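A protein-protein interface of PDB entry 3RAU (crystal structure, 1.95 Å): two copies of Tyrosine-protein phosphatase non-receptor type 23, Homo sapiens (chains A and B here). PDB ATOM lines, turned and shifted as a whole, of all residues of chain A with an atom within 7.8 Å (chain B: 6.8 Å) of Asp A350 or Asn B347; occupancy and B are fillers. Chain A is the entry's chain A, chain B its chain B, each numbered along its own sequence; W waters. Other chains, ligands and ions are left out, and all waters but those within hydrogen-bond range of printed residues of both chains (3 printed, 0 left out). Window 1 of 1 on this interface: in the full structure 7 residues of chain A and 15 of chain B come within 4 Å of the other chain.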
ATOM      1  N   ARG A  71     -19.128 -38.813   8.856  1.00  0.00           N
ATOM      2  CA  ARG A  71     -18.958 -37.397   9.181  1.00  0.00           C
ATOM      3  C   ARG A  71     -17.492 -37.068   9.416  1.00  0.00           C
ATOM      4  O   ARG A  71     -17.008 -36.022   8.988  1.00  0.00           O
ATOM      5  CB  ARG A  71     -19.789 -37.000  10.408  1.00  0.00           C
ATOM      6  CG  ARG A  71     -21.289 -37.029  10.148  1.00  0.00           C
ATOM      7  CD  ARG A  71     -22.078 -36.223  11.170  1.00  0.00           C
ATOM      8  NE  ARG A  71     -23.494 -36.199  10.812  1.00  0.00           N
ATOM      9  CZ  ARG A  71     -24.419 -36.997  11.336  1.00  0.00           C
ATOM     10  NH1 ARG A  71     -24.098 -37.877  12.273  1.00  0.00           N
ATOM     11  NH2 ARG A  71     -25.669 -36.903  10.927  1.00  0.00           N
ATOM     12  N   LYS A  72     -16.794 -37.961  10.095  1.00  0.00           N
ATOM     13  CA  LYS A  72     -15.372 -37.746  10.345  1.00  0.00           C
ATOM     14  C   LYS A  72     -14.607 -37.646   9.043  1.00  0.00           C
ATOM     15  O   LYS A  72     -13.785 -36.745   8.871  1.00  0.00           O
ATOM     16  CB  LYS A  72     -14.787 -38.860  11.198  1.00  0.00           C
ATOM     17  CG  LYS A  72     -13.269 -38.718  11.372  1.00  0.00           C
ATOM     18  CD  LYS A  72     -12.710 -39.666  12.415  1.00  0.00           C
ATOM     19  CE  LYS A  72     -11.272 -39.267  12.753  1.00  0.00           C
ATOM     20  NZ  LYS A  72     -10.682 -40.082  13.841  1.00  0.00           N
ATOM     21  N   GLY A  75     -15.407 -34.404   7.044  1.00  0.00           N
ATOM     22  CA  GLY A  75     -14.713 -33.265   7.618  1.00  0.00           C
ATOM     23  C   GLY A  75     -13.229 -33.251   7.281  1.00  0.00           C
ATOM     24  O   GLY A  75     -12.691 -32.203   6.909  1.00  0.00           O
ATOM     25  N   TYR A  79     -10.710 -30.427   5.514  1.00  0.00           N
ATOM     26  CA  TYR A  79      -9.396 -30.040   6.055  1.00  0.00           C
ATOM     27  C   TYR A  79      -8.302 -30.225   5.009  1.00  0.00           C
ATOM     28  O   TYR A  79      -7.458 -29.346   4.821  1.00  0.00           O
ATOM     29  CB  TYR A  79      -9.055 -30.852   7.304  1.00  0.00           C
ATOM     30  CG  TYR A  79     -10.002 -30.602   8.466  1.00  0.00           C
ATOM     31  CD1 TYR A  79     -10.751 -29.428   8.537  1.00  0.00           C
ATOM     32  CD2 TYR A  79     -10.132 -31.527   9.496  1.00  0.00           C
ATOM     33  CE1 TYR A  79     -11.621 -29.183   9.600  1.00  0.00           C
ATOM     34  CE2 TYR A  79     -11.000 -31.293  10.569  1.00  0.00           C
ATOM     35  CZ  TYR A  79     -11.740 -30.121  10.611  1.00  0.00           C
ATOM     36  OH  TYR A  79     -12.606 -29.885  11.661  1.00  0.00           O
ATOM     37  N   PRO A 345     -29.814 -29.596   9.474  1.00  0.00           N
ATOM     38  CA  PRO A 345     -28.575 -29.071   8.885  1.00  0.00           C
ATOM     39  C   PRO A 345     -27.359 -29.920   9.235  1.00  0.00           C
ATOM     40  O   PRO A 345     -27.347 -30.552  10.285  1.00  0.00           O
ATOM     41  CB  PRO A 345     -28.450 -27.682   9.522  1.00  0.00           C
ATOM     42  CG  PRO A 345     -29.154 -27.811  10.839  1.00  0.00           C
ATOM     43  CD  PRO A 345     -30.286 -28.779  10.608  1.00  0.00           C
ATOM     44  N   VAL A 346     -26.360 -29.935   8.357  1.00  0.00           N
ATOM     45  CA  VAL A 346     -25.099 -30.620   8.620  1.00  0.00           C
ATOM     46  C   VAL A 346     -23.988 -29.582   8.716  1.00  0.00           C
ATOM     47  O   VAL A 346     -23.922 -28.682   7.875  1.00  0.00           O
ATOM     48  CB  VAL A 346     -24.719 -31.550   7.456  1.00  0.00           C
ATOM     49  CG1 VAL A 346     -23.728 -32.609   7.925  1.00  0.00           C
ATOM     50  CG2 VAL A 346     -25.962 -32.180   6.830  1.00  0.00           C
ATOM     51  N   ASN A 347     -23.137 -29.674   9.739  1.00  0.00           N
ATOM     52  CA  ASN A 347     -21.880 -28.909   9.720  1.00  0.00           C
ATOM     53  C   ASN A 347     -20.722 -29.849   9.448  1.00  0.00           C
ATOM     54  O   ASN A 347     -20.308 -30.606  10.322  1.00  0.00           O
ATOM     55  CB  ASN A 347     -21.636 -28.119  11.009  1.00  0.00           C
ATOM     56  CG  ASN A 347     -20.234 -27.484  11.061  1.00  0.00           C
ATOM     57  OD1 ASN A 347     -19.729 -27.172  12.144  1.00  0.00           O
ATOM     58  ND2 ASN A 347     -19.601 -27.303   9.893  1.00  0.00           N
ATOM     59  N   PRO A 348     -20.201 -29.815   8.219  1.00  0.00           N
ATOM     60  CA  PRO A 348     -19.208 -30.827   7.856  1.00  0.00           C
ATOM     61  C   PRO A 348     -17.935 -30.686   8.677  1.00  0.00           C
ATOM     62  O   PRO A 348     -17.203 -31.664   8.835  1.00  0.00           O
ATOM     63  CB  PRO A 348     -18.940 -30.541   6.375  1.00  0.00           C
ATOM     64  CG  PRO A 348     -20.143 -29.789   5.903  1.00  0.00           C
ATOM     65  CD  PRO A 348     -20.561 -28.955   7.079  1.00  0.00           C
ATOM     66  N   THR A 349     -17.671 -29.495   9.211  1.00  0.00           N
ATOM     67  CA  THR A 349     -16.404 -29.281   9.888  1.00  0.00           C
ATOM     68  C   THR A 349     -16.540 -29.047  11.396  1.00  0.00           C
ATOM     69  O   THR A 349     -15.667 -28.445  12.027  1.00  0.00           O
ATOM     70  CB  THR A 349     -15.562 -28.177   9.194  1.00  0.00           C
ATOM     71  OG1 THR A 349     -16.312 -26.955   9.122  1.00  0.00           O
ATOM     72  CG2 THR A 349     -15.203 -28.622   7.776  1.00  0.00           C
ATOM     73  N   ASP A 350     -17.626 -29.545  11.973  1.00  0.00           N
ATOM     74  CA  ASP A 350     -17.773 -29.545  13.429  1.00  0.00           C
ATOM     75  C   ASP A 350     -16.628 -30.332  14.086  1.00  0.00           C
ATOM     76  O   ASP A 350     -16.532 -31.542  13.923  1.00  0.00           O
ATOM     77  CB  ASP A 350     -19.119 -30.141  13.826  1.00  0.00           C
ATOM     78  CG  ASP A 350     -19.346 -30.114  15.331  1.00  0.00           C
ATOM     79  OD1 ASP A 350     -18.419 -29.725  16.074  1.00  0.00           O
ATOM     80  OD2 ASP A 350     -20.449 -30.499  15.767  1.00  0.00           O
ATOM     81  N   PRO A 351     -15.747 -29.639  14.832  1.00  0.00           N
ATOM     82  CA  PRO A 351     -14.597 -30.305  15.461  1.00  0.00           C
ATOM     83  C   PRO A 351     -15.011 -31.487  16.335  1.00  0.00           C
ATOM     84  O   PRO A 351     -14.228 -32.415  16.535  1.00  0.00           O
ATOM     85  CB  PRO A 351     -13.985 -29.200  16.324  1.00  0.00           C
ATOM     86  CG  PRO A 351     -14.367 -27.935  15.624  1.00  0.00           C
ATOM     87  CD  PRO A 351     -15.753 -28.189  15.081  1.00  0.00           C
ATOM     88  N   ALA A 352     -16.237 -31.442  16.847  1.00  0.00           N
ATOM     89  CA  ALA A 352     -16.753 -32.511  17.688  1.00  0.00           C
ATOM     90  C   ALA A 352     -16.856 -33.829  16.921  1.00  0.00           C
ATOM     91  O   ALA A 352     -16.645 -34.898  17.491  1.00  0.00           O
ATOM     92  CB  ALA A 352     -18.105 -32.122  18.269  1.00  0.00           C
ATOM     93  N   VAL A 353     -17.173 -33.754  15.630  1.00  0.00           N
ATOM     94  CA  VAL A 353     -17.301 -34.969  14.822  1.00  0.00           C
ATOM     95  C   VAL A 353     -15.993 -35.370  14.126  1.00  0.00           C
ATOM     96  O   VAL A 353     -15.708 -36.562  13.985  1.00  0.00           O
ATOM     97  CB  VAL A 353     -18.432 -34.867  13.762  1.00  0.00           C
ATOM     98  CG1 VAL A 353     -19.706 -34.299  14.380  1.00  0.00           C
ATOM     99  CG2 VAL A 353     -17.982 -34.027  12.570  1.00  0.00           C
ATOM    100  N   THR A 354     -15.193 -34.385  13.706  1.00  0.00           N
ATOM    101  CA  THR A 354     -13.995 -34.671  12.924  1.00  0.00           C
ATOM    102  C   THR A 354     -12.805 -35.078  13.774  1.00  0.00           C
ATOM    103  O   THR A 354     -11.921 -35.795  13.307  1.00  0.00           O
ATOM    104  CB  THR A 354     -13.540 -33.448  12.088  1.00  0.00           C
ATOM    105  OG1 THR A 354     -13.061 -32.404  12.962  1.00  0.00           O
ATOM    106  CG2 THR A 354     -14.682 -32.933  11.231  1.00  0.00           C
ATOM    107  N   GLY A 355     -12.768 -34.599  15.013  1.00  0.00           N
ATOM    108  CA  GLY A 355     -11.570 -34.724  15.822  1.00  0.00           C
ATOM    109  C   GLY A 355     -10.502 -33.809  15.251  1.00  0.00           C
ATOM    110  O   GLY A 355     -10.790 -33.006  14.355  1.00  0.00           O
ATOM    111  N   ARG B  71     -24.450 -22.182  26.740  1.00  0.00           N
ATOM    112  CA  ARG B  71     -24.658 -23.210  25.734  1.00  0.00           C
ATOM    113  C   ARG B  71     -25.963 -23.971  25.967  1.00  0.00           C
ATOM    114  O   ARG B  71     -26.644 -24.328  25.017  1.00  0.00           O
ATOM    115  CB  ARG B  71     -23.473 -24.180  25.671  1.00  0.00           C
ATOM    116  CG  ARG B  71     -22.214 -23.544  25.106  1.00  0.00           C
ATOM    117  CD  ARG B  71     -21.181 -24.562  24.655  1.00  0.00           C
ATOM    118  NE  ARG B  71     -20.149 -23.905  23.855  1.00  0.00           N
ATOM    119  CZ  ARG B  71     -18.924 -23.609  24.286  1.00  0.00           C
ATOM    120  NH1 ARG B  71     -18.543 -23.937  25.514  1.00  0.00           N
ATOM    121  NH2 ARG B  71     -18.075 -23.000  23.473  1.00  0.00           N
ATOM    122  N   LEU B  74     -28.878 -21.629  24.950  1.00  0.00           N
ATOM    123  CA  LEU B  74     -28.885 -21.476  23.507  1.00  0.00           C
ATOM    124  C   LEU B  74     -29.537 -22.692  22.840  1.00  0.00           C
ATOM    125  O   LEU B  74     -30.349 -22.543  21.935  1.00  0.00           O
ATOM    126  CB  LEU B  74     -27.453 -21.243  22.971  1.00  0.00           C
ATOM    127  CG  LEU B  74     -27.310 -21.074  21.449  1.00  0.00           C
ATOM    128  CD1 LEU B  74     -28.109 -19.886  20.925  1.00  0.00           C
ATOM    129  CD2 LEU B  74     -25.845 -20.948  21.032  1.00  0.00           C
ATOM    130  N   GLY B  75     -29.178 -23.892  23.290  1.00  0.00           N
ATOM    131  CA  GLY B  75     -29.726 -25.107  22.717  1.00  0.00           C
ATOM    132  C   GLY B  75     -31.211 -25.244  22.999  1.00  0.00           C
ATOM    133  O   GLY B  75     -31.983 -25.643  22.125  1.00  0.00           O
ATOM    134  N   TYR B 158     -19.697 -17.919  13.828  1.00  0.00           N
ATOM    135  CA  TYR B 158     -20.983 -18.578  13.609  1.00  0.00           C
ATOM    136  C   TYR B 158     -22.059 -17.508  13.428  1.00  0.00           C
ATOM    137  O   TYR B 158     -22.904 -17.590  12.528  1.00  0.00           O
ATOM    138  CB  TYR B 158     -21.299 -19.496  14.792  1.00  0.00           C
ATOM    139  CG  TYR B 158     -22.576 -20.278  14.639  1.00  0.00           C
ATOM    140  CD1 TYR B 158     -22.554 -21.599  14.218  1.00  0.00           C
ATOM    141  CD2 TYR B 158     -23.805 -19.691  14.901  1.00  0.00           C
ATOM    142  CE1 TYR B 158     -23.732 -22.328  14.079  1.00  0.00           C
ATOM    143  CE2 TYR B 158     -24.991 -20.409  14.761  1.00  0.00           C
ATOM    144  CZ  TYR B 158     -24.944 -21.726  14.349  1.00  0.00           C
ATOM    145  OH  TYR B 158     -26.110 -22.444  14.206  1.00  0.00           O
ATOM    146  N   LYS B 342      -7.944 -21.966  14.713  1.00  0.00           N
ATOM    147  CA  LYS B 342      -9.115 -21.730  13.872  1.00  0.00           C
ATOM    148  C   LYS B 342     -10.329 -21.398  14.743  1.00  0.00           C
ATOM    149  O   LYS B 342     -10.336 -21.693  15.935  1.00  0.00           O
ATOM    150  CB  LYS B 342      -9.396 -22.960  12.999  1.00  0.00           C
ATOM    151  CG  LYS B 342      -9.718 -24.224  13.796  1.00  0.00           C
ATOM    152  CD  LYS B 342     -10.155 -25.361  12.876  1.00  0.00           C
ATOM    153  CE  LYS B 342     -10.278 -26.669  13.631  1.00  0.00           C
ATOM    154  NZ  LYS B 342     -10.674 -27.798  12.720  1.00  0.00           N
ATOM    155  N   PRO B 345     -16.298 -23.722  15.987  1.00  0.00           N
ATOM    156  CA  PRO B 345     -17.741 -23.494  15.856  1.00  0.00           C
ATOM    157  C   PRO B 345     -18.519 -24.239  16.933  1.00  0.00           C
ATOM    158  O   PRO B 345     -18.080 -25.278  17.409  1.00  0.00           O
ATOM    159  CB  PRO B 345     -18.075 -24.097  14.482  1.00  0.00           C
ATOM    160  CG  PRO B 345     -16.762 -24.336  13.809  1.00  0.00           C
ATOM    161  CD  PRO B 345     -15.777 -24.571  14.904  1.00  0.00           C
ATOM    162  N   VAL B 346     -19.666 -23.701  17.313  1.00  0.00           N
ATOM    163  CA  VAL B 346     -20.543 -24.401  18.225  1.00  0.00           C
ATOM    164  C   VAL B 346     -21.555 -25.158  17.397  1.00  0.00           C
ATOM    165  O   VAL B 346     -21.930 -24.722  16.305  1.00  0.00           O
ATOM    166  CB  VAL B 346     -21.298 -23.419  19.139  1.00  0.00           C
ATOM    167  CG1 VAL B 346     -20.321 -22.671  20.033  1.00  0.00           C
ATOM    168  CG2 VAL B 346     -22.100 -22.443  18.312  1.00  0.00           C
ATOM    169  N   ASN B 347     -21.972 -26.313  17.897  1.00  0.00           N
ATOM    170  CA  ASN B 347     -23.200 -26.931  17.432  1.00  0.00           C
ATOM    171  C   ASN B 347     -24.262 -26.610  18.483  1.00  0.00           C
ATOM    172  O   ASN B 347     -24.241 -27.181  19.575  1.00  0.00           O
ATOM    173  CB  ASN B 347     -23.018 -28.438  17.283  1.00  0.00           C
ATOM    174  CG  ASN B 347     -24.320 -29.154  16.969  1.00  0.00           C
ATOM    175  OD1 ASN B 347     -25.311 -28.527  16.582  1.00  0.00           O
ATOM    176  ND2 ASN B 347     -24.328 -30.472  17.137  1.00  0.00           N
ATOM    177  N   PRO B 348     -25.184 -25.687  18.165  1.00  0.00           N
ATOM    178  CA  PRO B 348     -26.166 -25.218  19.155  1.00  0.00           C
ATOM    179  C   PRO B 348     -26.984 -26.346  19.790  1.00  0.00           C
ATOM    180  O   PRO B 348     -27.371 -26.236  20.951  1.00  0.00           O
ATOM    181  CB  PRO B 348     -27.082 -24.300  18.336  1.00  0.00           C
ATOM    182  CG  PRO B 348     -26.253 -23.886  17.162  1.00  0.00           C
ATOM    183  CD  PRO B 348     -25.400 -25.079  16.842  1.00  0.00           C
ATOM    184  N   THR B 349     -27.221 -27.426  19.055  1.00  0.00           N
ATOM    185  CA  THR B 349     -28.069 -28.499  19.570  1.00  0.00           C
ATOM    186  C   THR B 349     -27.319 -29.793  19.889  1.00  0.00           C
ATOM    187  O   THR B 349     -27.884 -30.884  19.803  1.00  0.00           O
ATOM    188  CB  THR B 349     -29.230 -28.799  18.608  1.00  0.00           C
ATOM    189  OG1 THR B 349     -28.708 -29.070  17.298  1.00  0.00           O
ATOM    190  CG2 THR B 349     -30.148 -27.603  18.543  1.00  0.00           C
ATOM    191  N   ASP B 350     -26.049 -29.659  20.252  1.00  0.00           N
ATOM    192  CA  ASP B 350     -25.246 -30.781  20.734  1.00  0.00           C
ATOM    193  C   ASP B 350     -25.854 -31.315  22.037  1.00  0.00           C
ATOM    194  O   ASP B 350     -25.871 -30.624  23.053  1.00  0.00           O
ATOM    195  CB  ASP B 350     -23.814 -30.302  20.973  1.00  0.00           C
ATOM    196  CG  ASP B 350     -22.835 -31.442  21.155  1.00  0.00           C
ATOM    197  OD1 ASP B 350     -23.248 -32.516  21.639  1.00  0.00           O
ATOM    198  OD2 ASP B 350     -21.646 -31.254  20.816  1.00  0.00           O
ATOM    199  N   PRO B 351     -26.354 -32.556  22.022  1.00  0.00           N
ATOM    200  CA  PRO B 351     -27.066 -33.035  23.216  1.00  0.00           C
ATOM    201  C   PRO B 351     -26.179 -33.029  24.461  1.00  0.00           C
ATOM    202  O   PRO B 351     -26.680 -32.924  25.579  1.00  0.00           O
ATOM    203  CB  PRO B 351     -27.472 -34.462  22.833  1.00  0.00           C
ATOM    204  CG  PRO B 351     -27.519 -34.443  21.328  1.00  0.00           C
ATOM    205  CD  PRO B 351     -26.406 -33.520  20.912  1.00  0.00           C
ATOM    206  N   VAL B 353     -24.424 -30.647  25.488  1.00  0.00           N
ATOM    207  CA  VAL B 353     -24.419 -29.332  26.135  1.00  0.00           C
ATOM    208  C   VAL B 353     -25.819 -28.865  26.539  1.00  0.00           C
ATOM    209  O   VAL B 353     -25.975 -28.031  27.427  1.00  0.00           O
ATOM    210  CB  VAL B 353     -23.756 -28.241  25.243  1.00  0.00           C
ATOM    211  CG1 VAL B 353     -22.344 -28.655  24.839  1.00  0.00           C
ATOM    212  CG2 VAL B 353     -24.616 -27.938  24.011  1.00  0.00           C
ATOM    213  N   THR B 354     -26.839 -29.411  25.894  1.00  0.00           N
ATOM    214  CA  THR B 354     -28.203 -28.951  26.136  1.00  0.00           C
ATOM    215  C   THR B 354     -28.902 -29.647  27.290  1.00  0.00           C
ATOM    216  O   THR B 354     -29.785 -29.071  27.922  1.00  0.00           O
ATOM    217  CB  THR B 354     -29.074 -29.111  24.880  1.00  0.00           C
ATOM    218  OG1 THR B 354     -29.275 -30.500  24.616  1.00  0.00           O
ATOM    219  CG2 THR B 354     -28.399 -28.459  23.678  1.00  0.00           C
HETATM  220  O   HOH W   1     -13.343 -26.976  11.971  1.00  0.00           O
HETATM  221  O   HOH W   2     -21.844 -31.717  17.650  1.00  0.00           O
HETATM  222  O   HOH W   3     -10.559 -30.041  14.171  1.00  0.00           O
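Of the printed residues of chain B, Asp A350 touches Asn B347 (3.6 Å). Asn B347 touches just one residue of chain A: Asp A350. No residue of chain A comes within 4 Å of Pro B348. Printed residues of chain A within 4 Å of Pro B345: Pro A351. Of the printed residues of chain B, Tyr A79 touches Lys B342. The nearest residue of chain B that does not touch Asp A350 is Pro B345 (4.7 Å).
Water W2 lies within hydrogen-bond range of the side-chain carboxylate (OD2) of Asp A350, the side-chain amide nitrogen (ND2) of Asn B347 and the side-chain carboxylate (OD2) of Asp B350. Water W3 lies within hydrogen-bond range of the side-chain amino group (NZ) of Lys B342 (2.7 Å), the backbone carbonyl oxygen (O) of Gly A355 (3.0 Å) and the side-chain hydroxyl (OH) of Tyr A79 (3.2 Å). Water W1 lies within hydrogen-bond range of O of Thr A349, NZ of Lys B342 and OH of Tyr A79.
Asp A350 touches Asn B347, but with the chains exchanged Asn A347 does not touch Asp B350 (9.8 Å). Pro A351 touches Pro B345, but with the chains exchanged Pro A345 does not touch Pro B351 (11.1 Å). 11 positions are printed for both chains.
NZ of Lys B342 lies within hydrogen-bond range of OH of Tyr A79 (3.0 Å).
OH of Tyr A79 lies within hydrogen-bond range of O of Thr A349 (3.4 Å). OD1 of Asn B347 lies close to N of Thr B349 (3.3 Å). The backbone NH (N) of Ala A352 sits at hydrogen-bond distance from the side-chain carboxylate (OD1) of Asp A350. The backbone NH (N) of Asp A350 lies within hydrogen-bond range of the side-chain amide oxygen (OD1) of Asn A347 (3.2 Å). The side-chain hydroxyl of Tyr A79 lies within hydrogen-bond range of the side-chain hydroxyl of Thr A354 (2.9 Å).
Among the printed residues, merely in contact across the chains: Pro A351 with Pro B345 (3.6 Å) and Asp A350 with Asn B347 (3.6 Å).
Of the 15 printed residues of chain A, 3 touch a printed residue of chain B. Printed residues of chain A that touch a printed residue of chain B: Tyr A79, Asp A350 and Pro A351. Hydrophobic or aromatic side chains of chain A within 4 Å of the printed part of chain B: Tyr A79 and Pro A351. Among the printed residues, 3 pairs touch across the chains. Among the printed residues, no Asp or Glu carboxylate lies within 4 Å of a Lys or Arg side-chain nitrogen of the other chain.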
